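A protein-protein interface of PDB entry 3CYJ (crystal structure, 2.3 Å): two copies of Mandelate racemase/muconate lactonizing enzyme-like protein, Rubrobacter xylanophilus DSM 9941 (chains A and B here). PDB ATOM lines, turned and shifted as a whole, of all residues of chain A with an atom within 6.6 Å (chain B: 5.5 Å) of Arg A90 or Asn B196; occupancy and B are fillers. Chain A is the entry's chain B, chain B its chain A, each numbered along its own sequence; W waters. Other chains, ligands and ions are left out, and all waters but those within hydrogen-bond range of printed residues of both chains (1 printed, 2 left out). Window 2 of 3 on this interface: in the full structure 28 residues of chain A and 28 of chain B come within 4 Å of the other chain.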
ATOM      1  N   MET A  85     -14.212  -5.365   5.955  1.00  0.00           N
ATOM      2  CA  MET A  85     -13.804  -6.608   5.310  1.00  0.00           C
ATOM      3  C   MET A  85     -12.626  -6.349   4.343  1.00  0.00           C
ATOM      4  O   MET A  85     -11.598  -7.019   4.443  1.00  0.00           O
ATOM      5  CB  MET A  85     -15.008  -7.308   4.616  1.00  0.00           C
ATOM      6  CG  MET A  85     -16.016  -8.073   5.561  1.00  0.00           C
ATOM      7  SD  MET A  85     -17.207  -9.212   4.724  1.00  0.00           S
ATOM      8  CE  MET A  85     -18.226  -8.047   3.826  1.00  0.00           C
ATOM      9  N   GLN A  86     -12.754  -5.371   3.422  1.00  0.00           N
ATOM     10  CA  GLN A  86     -11.656  -4.991   2.511  1.00  0.00           C
ATOM     11  C   GLN A  86     -10.354  -4.640   3.251  1.00  0.00           C
ATOM     12  O   GLN A  86      -9.260  -4.944   2.763  1.00  0.00           O
ATOM     13  CB  GLN A  86     -12.043  -3.813   1.591  1.00  0.00           C
ATOM     14  CG  GLN A  86     -13.306  -3.983   0.768  1.00  0.00           C
ATOM     15  CD  GLN A  86     -13.157  -4.982  -0.403  1.00  0.00           C
ATOM     16  OE1 GLN A  86     -12.094  -5.631  -0.582  1.00  0.00           O
ATOM     17  NE2 GLN A  86     -14.232  -5.112  -1.205  1.00  0.00           N
ATOM     18  N   ALA A  87     -10.461  -3.995   4.426  1.00  0.00           N
ATOM     19  CA  ALA A  87      -9.243  -3.610   5.178  1.00  0.00           C
ATOM     20  C   ALA A  87      -8.624  -4.851   5.777  1.00  0.00           C
ATOM     21  O   ALA A  87      -7.392  -5.025   5.797  1.00  0.00           O
ATOM     22  CB  ALA A  87      -9.554  -2.575   6.285  1.00  0.00           C
ATOM     23  N   ALA A  88      -9.477  -5.744   6.253  1.00  0.00           N
ATOM     24  CA  ALA A  88      -9.021  -6.926   6.972  1.00  0.00           C
ATOM     25  C   ALA A  88      -8.250  -7.900   6.104  1.00  0.00           C
ATOM     26  O   ALA A  88      -7.410  -8.636   6.593  1.00  0.00           O
ATOM     27  CB  ALA A  88     -10.222  -7.628   7.674  1.00  0.00           C
ATOM     28  N   ILE A  89      -8.517  -7.923   4.814  1.00  0.00           N
ATOM     29  CA  ILE A  89      -7.913  -8.952   4.004  1.00  0.00           C
ATOM     30  C   ILE A  89      -6.715  -8.418   3.174  1.00  0.00           C
ATOM     31  O   ILE A  89      -6.331  -9.037   2.196  1.00  0.00           O
ATOM     32  CB  ILE A  89      -8.977  -9.659   3.117  1.00  0.00           C
ATOM     33  CG1 ILE A  89      -9.577  -8.696   2.072  1.00  0.00           C
ATOM     34  CG2 ILE A  89     -10.118 -10.316   4.023  1.00  0.00           C
ATOM     35  CD1 ILE A  89     -10.536  -9.344   1.097  1.00  0.00           C
ATOM     36  N   ARG A  90      -6.113  -7.299   3.578  1.00  0.00           N
ATOM     37  CA  ARG A  90      -4.948  -6.763   2.854  1.00  0.00           C
ATOM     38  C   ARG A  90      -3.883  -7.838   2.599  1.00  0.00           C
ATOM     39  O   ARG A  90      -3.490  -8.068   1.459  1.00  0.00           O
ATOM     40  CB  ARG A  90      -4.307  -5.575   3.588  1.00  0.00           C
ATOM     41  CG  ARG A  90      -3.200  -4.787   2.732  1.00  0.00           C
ATOM     42  CD  ARG A  90      -2.354  -3.851   3.667  1.00  0.00           C
ATOM     43  NE  ARG A  90      -1.388  -4.641   4.453  1.00  0.00           N
ATOM     44  CZ  ARG A  90      -0.695  -4.190   5.499  1.00  0.00           C
ATOM     45  NH1 ARG A  90      -0.854  -2.932   5.899  1.00  0.00           N
ATOM     46  NH2 ARG A  90       0.138  -5.023   6.163  1.00  0.00           N
ATOM     47  N   ASN A  91      -3.398  -8.476   3.657  1.00  0.00           N
ATOM     48  CA  ASN A  91      -2.418  -9.555   3.526  1.00  0.00           C
ATOM     49  C   ASN A  91      -3.029 -10.845   2.977  1.00  0.00           C
ATOM     50  O   ASN A  91      -2.370 -11.590   2.283  1.00  0.00           O
ATOM     51  CB  ASN A  91      -1.759  -9.873   4.885  1.00  0.00           C
ATOM     52  CG  ASN A  91      -0.985  -8.708   5.444  1.00  0.00           C
ATOM     53  OD1 ASN A  91      -0.749  -7.672   4.746  1.00  0.00           O
ATOM     54  ND2 ASN A  91      -0.543  -8.853   6.732  1.00  0.00           N
ATOM     55  N   ALA A  92      -4.282 -11.132   3.309  1.00  0.00           N
ATOM     56  CA  ALA A  92      -4.884 -12.413   2.930  1.00  0.00           C
ATOM     57  C   ALA A  92      -5.135 -12.488   1.426  1.00  0.00           C
ATOM     58  O   ALA A  92      -5.153 -13.572   0.851  1.00  0.00           O
ATOM     59  CB  ALA A  92      -6.166 -12.666   3.749  1.00  0.00           C
ATOM     60  N   GLY A  93      -5.269 -11.339   0.759  1.00  0.00           N
ATOM     61  CA  GLY A  93      -5.427 -11.344  -0.711  1.00  0.00           C
ATOM     62  C   GLY A  93      -6.810 -10.823  -1.091  1.00  0.00           C
ATOM     63  O   GLY A  93      -7.819 -11.539  -0.996  1.00  0.00           O
ATOM     64  N   ARG A  94      -6.839  -9.569  -1.498  1.00  0.00           N
ATOM     65  CA  ARG A  94      -8.055  -8.872  -1.859  1.00  0.00           C
ATOM     66  C   ARG A  94      -8.685  -9.374  -3.150  1.00  0.00           C
ATOM     67  O   ARG A  94      -9.880  -9.587  -3.173  1.00  0.00           O
ATOM     68  CB  ARG A  94      -7.751  -7.385  -2.001  1.00  0.00           C
ATOM     69  CG  ARG A  94      -8.700  -6.488  -1.248  1.00  0.00           C
ATOM     70  CD  ARG A  94      -7.984  -5.184  -1.029  1.00  0.00           C
ATOM     71  NE  ARG A  94      -7.834  -4.811   0.367  1.00  0.00           N
ATOM     72  CZ  ARG A  94      -6.879  -3.987   0.789  1.00  0.00           C
ATOM     73  NH1 ARG A  94      -6.005  -3.482  -0.087  1.00  0.00           N
ATOM     74  NH2 ARG A  94      -6.793  -3.670   2.066  1.00  0.00           N
ATOM     75  N   ASP B  26       1.234  -1.887  11.348  1.00  0.00           N
ATOM     76  CA  ASP B  26       1.888  -1.010  10.422  1.00  0.00           C
ATOM     77  C   ASP B  26       0.841   0.055  10.153  1.00  0.00           C
ATOM     78  O   ASP B  26      -0.210   0.096  10.873  1.00  0.00           O
ATOM     79  CB  ASP B  26       2.383  -1.748   9.156  1.00  0.00           C
ATOM     80  CG  ASP B  26       1.268  -2.446   8.372  1.00  0.00           C
ATOM     81  OD1 ASP B  26       0.122  -1.928   8.326  1.00  0.00           O
ATOM     82  OD2 ASP B  26       1.548  -3.506   7.760  1.00  0.00           O
ATOM     83  N   GLY B  27       1.099   0.890   9.149  1.00  0.00           N
ATOM     84  CA  GLY B  27       0.205   1.982   8.868  1.00  0.00           C
ATOM     85  C   GLY B  27      -1.230   1.552   8.619  1.00  0.00           C
ATOM     86  O   GLY B  27      -2.123   2.262   8.964  1.00  0.00           O
ATOM     87  N   THR B  28      -1.484   0.397   8.034  1.00  0.00           N
ATOM     88  CA  THR B  28      -2.856   0.066   7.720  1.00  0.00           C
ATOM     89  C   THR B  28      -3.340  -1.299   8.266  1.00  0.00           C
ATOM     90  O   THR B  28      -4.414  -1.757   7.863  1.00  0.00           O
ATOM     91  CB  THR B  28      -3.102   0.094   6.138  1.00  0.00           C
ATOM     92  OG1 THR B  28      -2.079  -0.662   5.485  1.00  0.00           O
ATOM     93  CG2 THR B  28      -3.075   1.489   5.567  1.00  0.00           C
ATOM     94  N   LEU B  29      -2.588  -1.953   9.153  1.00  0.00           N
ATOM     95  CA  LEU B  29      -3.005  -3.277   9.621  1.00  0.00           C
ATOM     96  C   LEU B  29      -2.383  -3.687  10.973  1.00  0.00           C
ATOM     97  O   LEU B  29      -1.312  -3.211  11.332  1.00  0.00           O
ATOM     98  CB  LEU B  29      -2.749  -4.324   8.545  1.00  0.00           C
ATOM     99  CG  LEU B  29      -3.435  -5.704   8.654  1.00  0.00           C
ATOM    100  CD1 LEU B  29      -4.864  -5.680   8.229  1.00  0.00           C
ATOM    101  CD2 LEU B  29      -2.720  -6.709   7.795  1.00  0.00           C
ATOM    102  N   TRP B  31      -1.759  -7.272  13.485  1.00  0.00           N
ATOM    103  CA  TRP B  31      -1.791  -8.714  13.473  1.00  0.00           C
ATOM    104  C   TRP B  31      -0.988  -9.229  14.650  1.00  0.00           C
ATOM    105  O   TRP B  31      -0.194  -8.505  15.208  1.00  0.00           O
ATOM    106  CB  TRP B  31      -1.287  -9.303  12.114  1.00  0.00           C
ATOM    107  CG  TRP B  31       0.164  -9.016  11.812  1.00  0.00           C
ATOM    108  CD1 TRP B  31       1.218  -9.898  11.923  1.00  0.00           C
ATOM    109  CD2 TRP B  31       0.732  -7.770  11.347  1.00  0.00           C
ATOM    110  NE1 TRP B  31       2.390  -9.275  11.548  1.00  0.00           N
ATOM    111  CE2 TRP B  31       2.130  -7.974  11.205  1.00  0.00           C
ATOM    112  CE3 TRP B  31       0.189  -6.516  11.013  1.00  0.00           C
ATOM    113  CZ2 TRP B  31       3.015  -6.952  10.764  1.00  0.00           C
ATOM    114  CZ3 TRP B  31       1.062  -5.496  10.576  1.00  0.00           C
ATOM    115  CH2 TRP B  31       2.471  -5.733  10.458  1.00  0.00           C
ATOM    116  N   LYS B 166       8.367   0.774  10.137  1.00  0.00           N
ATOM    117  CA  LYS B 166       7.053   1.278   9.782  1.00  0.00           C
ATOM    118  C   LYS B 166       6.792   2.700  10.267  1.00  0.00           C
ATOM    119  O   LYS B 166       7.237   3.113  11.339  1.00  0.00           O
ATOM    120  CB  LYS B 166       5.983   0.345  10.340  1.00  0.00           C
ATOM    121  CG  LYS B 166       6.209  -1.154  10.085  1.00  0.00           C
ATOM    122  CD  LYS B 166       6.322  -1.452   8.615  1.00  0.00           C
ATOM    123  CE  LYS B 166       5.858  -2.857   8.323  1.00  0.00           C
ATOM    124  NZ  LYS B 166       6.439  -3.306   7.048  1.00  0.00           N
ATOM    125  N   VAL B 167       6.067   3.459   9.447  1.00  0.00           N
ATOM    126  CA  VAL B 167       5.616   4.815   9.783  1.00  0.00           C
ATOM    127  C   VAL B 167       4.169   4.959   9.334  1.00  0.00           C
ATOM    128  O   VAL B 167       3.662   4.164   8.531  1.00  0.00           O
ATOM    129  CB  VAL B 167       6.412   5.950   8.996  1.00  0.00           C
ATOM    130  CG1 VAL B 167       7.800   6.096   9.507  1.00  0.00           C
ATOM    131  CG2 VAL B 167       6.367   5.686   7.456  1.00  0.00           C
ATOM    132  N   ASP B 194       8.468   2.336   5.639  1.00  0.00           N
ATOM    133  CA  ASP B 194       7.386   1.710   4.937  1.00  0.00           C
ATOM    134  C   ASP B 194       6.081   2.249   5.522  1.00  0.00           C
ATOM    135  O   ASP B 194       5.870   2.149   6.721  1.00  0.00           O
ATOM    136  CB  ASP B 194       7.497   0.188   5.047  1.00  0.00           C
ATOM    137  CG  ASP B 194       6.410  -0.552   4.255  1.00  0.00           C
ATOM    138  OD1 ASP B 194       5.493   0.045   3.600  1.00  0.00           O
ATOM    139  OD2 ASP B 194       6.421  -1.784   4.332  1.00  0.00           O
ATOM    140  N   ALA B 195       5.213   2.804   4.659  1.00  0.00           N
ATOM    141  CA  ALA B 195       3.971   3.460   5.114  1.00  0.00           C
ATOM    142  C   ALA B 195       2.760   2.528   4.897  1.00  0.00           C
ATOM    143  O   ALA B 195       1.650   2.793   5.401  1.00  0.00           O
ATOM    144  CB  ALA B 195       3.773   4.797   4.389  1.00  0.00           C
ATOM    145  N   ASN B 196       2.981   1.441   4.146  1.00  0.00           N
ATOM    146  CA  ASN B 196       1.929   0.466   3.862  1.00  0.00           C
ATOM    147  C   ASN B 196       0.639   1.164   3.426  1.00  0.00           C
ATOM    148  O   ASN B 196      -0.461   0.850   3.947  1.00  0.00           O
ATOM    149  CB  ASN B 196       1.674  -0.419   5.111  1.00  0.00           C
ATOM    150  CG  ASN B 196       2.851  -1.348   5.399  1.00  0.00           C
ATOM    151  OD1 ASN B 196       2.880  -2.455   4.863  1.00  0.00           O
ATOM    152  ND2 ASN B 196       3.877  -0.865   6.154  1.00  0.00           N
ATOM    153  N   GLY B 197       0.793   2.138   2.529  1.00  0.00           N
ATOM    154  CA  GLY B 197      -0.331   2.876   1.935  1.00  0.00           C
ATOM    155  C   GLY B 197      -1.104   3.806   2.861  1.00  0.00           C
ATOM    156  O   GLY B 197      -2.254   4.138   2.587  1.00  0.00           O
ATOM    157  N   ALA B 198      -0.467   4.250   3.940  1.00  0.00           N
ATOM    158  CA  ALA B 198      -1.173   5.011   4.967  1.00  0.00           C
ATOM    159  C   ALA B 198      -1.529   6.452   4.630  1.00  0.00           C
ATOM    160  O   ALA B 198      -2.387   7.033   5.309  1.00  0.00           O
ATOM    161  CB  ALA B 198      -0.373   4.962   6.299  1.00  0.00           C
ATOM    162  N   GLU B 221       8.629   3.354   1.130  1.00  0.00           N
ATOM    163  CA  GLU B 221       7.848   2.305   0.534  1.00  0.00           C
ATOM    164  C   GLU B 221       6.315   2.504   0.721  1.00  0.00           C
ATOM    165  O   GLU B 221       5.835   2.852   1.814  1.00  0.00           O
ATOM    166  CB  GLU B 221       8.277   0.968   1.108  1.00  0.00           C
ATOM    167  CG  GLU B 221       7.666  -0.170   0.336  1.00  0.00           C
ATOM    168  CD  GLU B 221       7.884  -1.517   1.030  1.00  0.00           C
ATOM    169  OE1 GLU B 221       8.883  -1.648   1.798  1.00  0.00           O
ATOM    170  OE2 GLU B 221       7.040  -2.430   0.808  1.00  0.00           O
ATOM    171  N   GLU B 222       5.562   2.278  -0.361  1.00  0.00           N
ATOM    172  CA  GLU B 222       4.105   2.318  -0.304  1.00  0.00           C
ATOM    173  C   GLU B 222       3.544   3.560   0.375  1.00  0.00           C
ATOM    174  O   GLU B 222       2.683   3.461   1.261  1.00  0.00           O
ATOM    175  CB  GLU B 222       3.570   1.062   0.372  1.00  0.00           C
ATOM    176  CG  GLU B 222       3.658  -0.161  -0.569  1.00  0.00           C
ATOM    177  CD  GLU B 222       3.269  -1.510   0.097  1.00  0.00           C
ATOM    178  OE1 GLU B 222       3.036  -1.555   1.329  1.00  0.00           O
ATOM    179  OE2 GLU B 222       3.220  -2.543  -0.620  1.00  0.00           O
ATOM    180  N   PRO B 223       3.985   4.745  -0.094  1.00  0.00           N
ATOM    181  CA  PRO B 223       3.503   5.941   0.583  1.00  0.00           C
ATOM    182  C   PRO B 223       1.973   6.066   0.393  1.00  0.00           C
ATOM    183  O   PRO B 223       1.280   6.528   1.304  1.00  0.00           O
ATOM    184  CB  PRO B 223       4.227   7.070  -0.132  1.00  0.00           C
ATOM    185  CG  PRO B 223       4.550   6.506  -1.556  1.00  0.00           C
ATOM    186  CD  PRO B 223       4.778   5.031  -1.334  1.00  0.00           C
ATOM    187  N   GLU B 249       4.540  -5.215  -3.796  1.00  0.00           N
ATOM    188  CA  GLU B 249       4.017  -6.539  -3.338  1.00  0.00           C
ATOM    189  C   GLU B 249       2.673  -7.117  -3.872  1.00  0.00           C
ATOM    190  O   GLU B 249       2.484  -8.329  -3.847  1.00  0.00           O
ATOM    191  CB  GLU B 249       3.983  -6.623  -1.828  1.00  0.00           C
ATOM    192  CG  GLU B 249       3.361  -5.396  -1.167  1.00  0.00           C
ATOM    193  CD  GLU B 249       3.062  -5.648   0.272  1.00  0.00           C
ATOM    194  OE1 GLU B 249       3.157  -4.717   1.112  1.00  0.00           O
ATOM    195  OE2 GLU B 249       2.734  -6.815   0.566  1.00  0.00           O
ATOM    196  N   TYR B 250       1.743  -6.304  -4.348  1.00  0.00           N
ATOM    197  CA  TYR B 250       0.423  -6.873  -4.628  1.00  0.00           C
ATOM    198  C   TYR B 250       0.081  -7.145  -6.075  1.00  0.00           C
ATOM    199  O   TYR B 250      -1.057  -7.458  -6.356  1.00  0.00           O
ATOM    200  CB  TYR B 250      -0.673  -6.009  -4.015  1.00  0.00           C
ATOM    201  CG  TYR B 250      -0.504  -5.831  -2.515  1.00  0.00           C
ATOM    202  CD1 TYR B 250      -0.631  -6.919  -1.644  1.00  0.00           C
ATOM    203  CD2 TYR B 250      -0.198  -4.589  -1.971  1.00  0.00           C
ATOM    204  CE1 TYR B 250      -0.477  -6.745  -0.250  1.00  0.00           C
ATOM    205  CE2 TYR B 250      -0.053  -4.420  -0.599  1.00  0.00           C
ATOM    206  CZ  TYR B 250      -0.188  -5.493   0.252  1.00  0.00           C
ATOM    207  OH  TYR B 250      -0.014  -5.320   1.605  1.00  0.00           O
ATOM    208  N   ARG B 273       4.163 -14.675  -3.865  1.00  0.00           N
ATOM    209  CA  ARG B 273       2.916 -14.106  -4.359  1.00  0.00           C
ATOM    210  C   ARG B 273       2.918 -13.884  -5.847  1.00  0.00           C
ATOM    211  O   ARG B 273       1.871 -13.954  -6.470  1.00  0.00           O
ATOM    212  CB  ARG B 273       2.658 -12.762  -3.706  1.00  0.00           C
ATOM    213  CG  ARG B 273       2.329 -12.815  -2.265  1.00  0.00           C
ATOM    214  CD  ARG B 273       2.272 -11.444  -1.796  1.00  0.00           C
ATOM    215  NE  ARG B 273       1.600 -11.374  -0.538  1.00  0.00           N
ATOM    216  CZ  ARG B 273       1.643 -10.302   0.236  1.00  0.00           C
ATOM    217  NH1 ARG B 273       2.344  -9.228  -0.170  1.00  0.00           N
ATOM    218  NH2 ARG B 273       0.978 -10.298   1.396  1.00  0.00           N
HETATM  219  O   HOH W   1      -5.428  -2.830   5.533  1.00  0.00           O
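Leu B29 touches Ala A87 (CD1 to O, 3.6 Å). NH1 of Arg A90 touches CB of Leu B29, 3.5 Å away. Arg A90 touches Asn B196 (NH1 to CB, 3.7 Å). Asn A91 touches Leu B29 (ND2 to CD2, 3.2 Å). Asn A91 touches Tyr B250 (OD1 to OH, 3.99 Å). Asn A91 touches Arg B273 (O to NH2, 3.7 Å).
Of chain B, only Asp B26 (2.6 Å), Thr B28 (2.6 Å), Leu B29 (3.5 Å), Asn B196 (3.7 Å) and Tyr B250 (3.2 Å) come within 4 Å of Arg A90. Gly B27 touches none of the printed residues of chain A. Of the printed residues of chain A, Leu B29 touches Ala A87, Arg A90 and Asn A91. Asn B196 touches just one residue of chain A: Arg A90. Of the printed residues of chain A, Arg B273 touches Asn A91. The nearest residue of chain B that does not touch Arg A90 is Trp B31 (4.5 Å). The nearest residue of chain A that does not touch Asn B196 is Asn A91 (6.4 Å). The nearest printed residue of chain B that does not touch Asn A91 is Trp B31 (4.9 Å).
The side-chain hydroxyl of Tyr B250 is in hydrogen-bond range of the guanidinium group of Arg A90 (3.2 Å). The guanidinium group of Arg A90 lies within salt-bridge range of the side-chain carboxylate of Asp B26 (2.6 Å). The side-chain hydroxyl of Thr B28 sits at hydrogen-bond distance from the guanidinium group of Arg A90 (2.6 Å).
No position is printed for both chains. Of the 9 pairs that touch across the chains among the printed residues, none has its exchanged pair printed and touching as well.
The side-chain amide oxygen of Asn A91 is in hydrogen-bond range of the guanidinium group of Arg A90 (3.1 Å). The backbone NH (N) of Asn B196 lies within hydrogen-bond range of the side-chain carboxylate (OD1) of Asp B194. OD2 of Asp B26 lies close to OD1 of Asn B196 (3.4 Å). The side-chain carboxylate (OD1) of Asp B26 sits at hydrogen-bond distance from the backbone NH (N) of Leu B29. The side-chain carboxylate of Glu B249 is in salt-bridge range of the guanidinium group of Arg B273. OE1 of Glu B249 is in hydrogen-bond range of OH of Tyr B250 (3.3 Å).
Along chain A the printed residues that touch a printed residue of chain B span positions 87 to 91. Of the 18 printed residues of chain B, 6 touch a printed residue of chain A. Hydrophobic or aromatic side chains of chain B within 4 Å of the printed part of chain A: Leu B29 and Tyr B250. Among the printed residues, 9 pairs touch across the chains.
Water W1 lies within hydrogen-bond range of the backbone carbonyl oxygen (O) of Thr B28 (2.8 Å) and the backbone carbonyl oxygen (O) of Ala A87 (3.0 Å).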
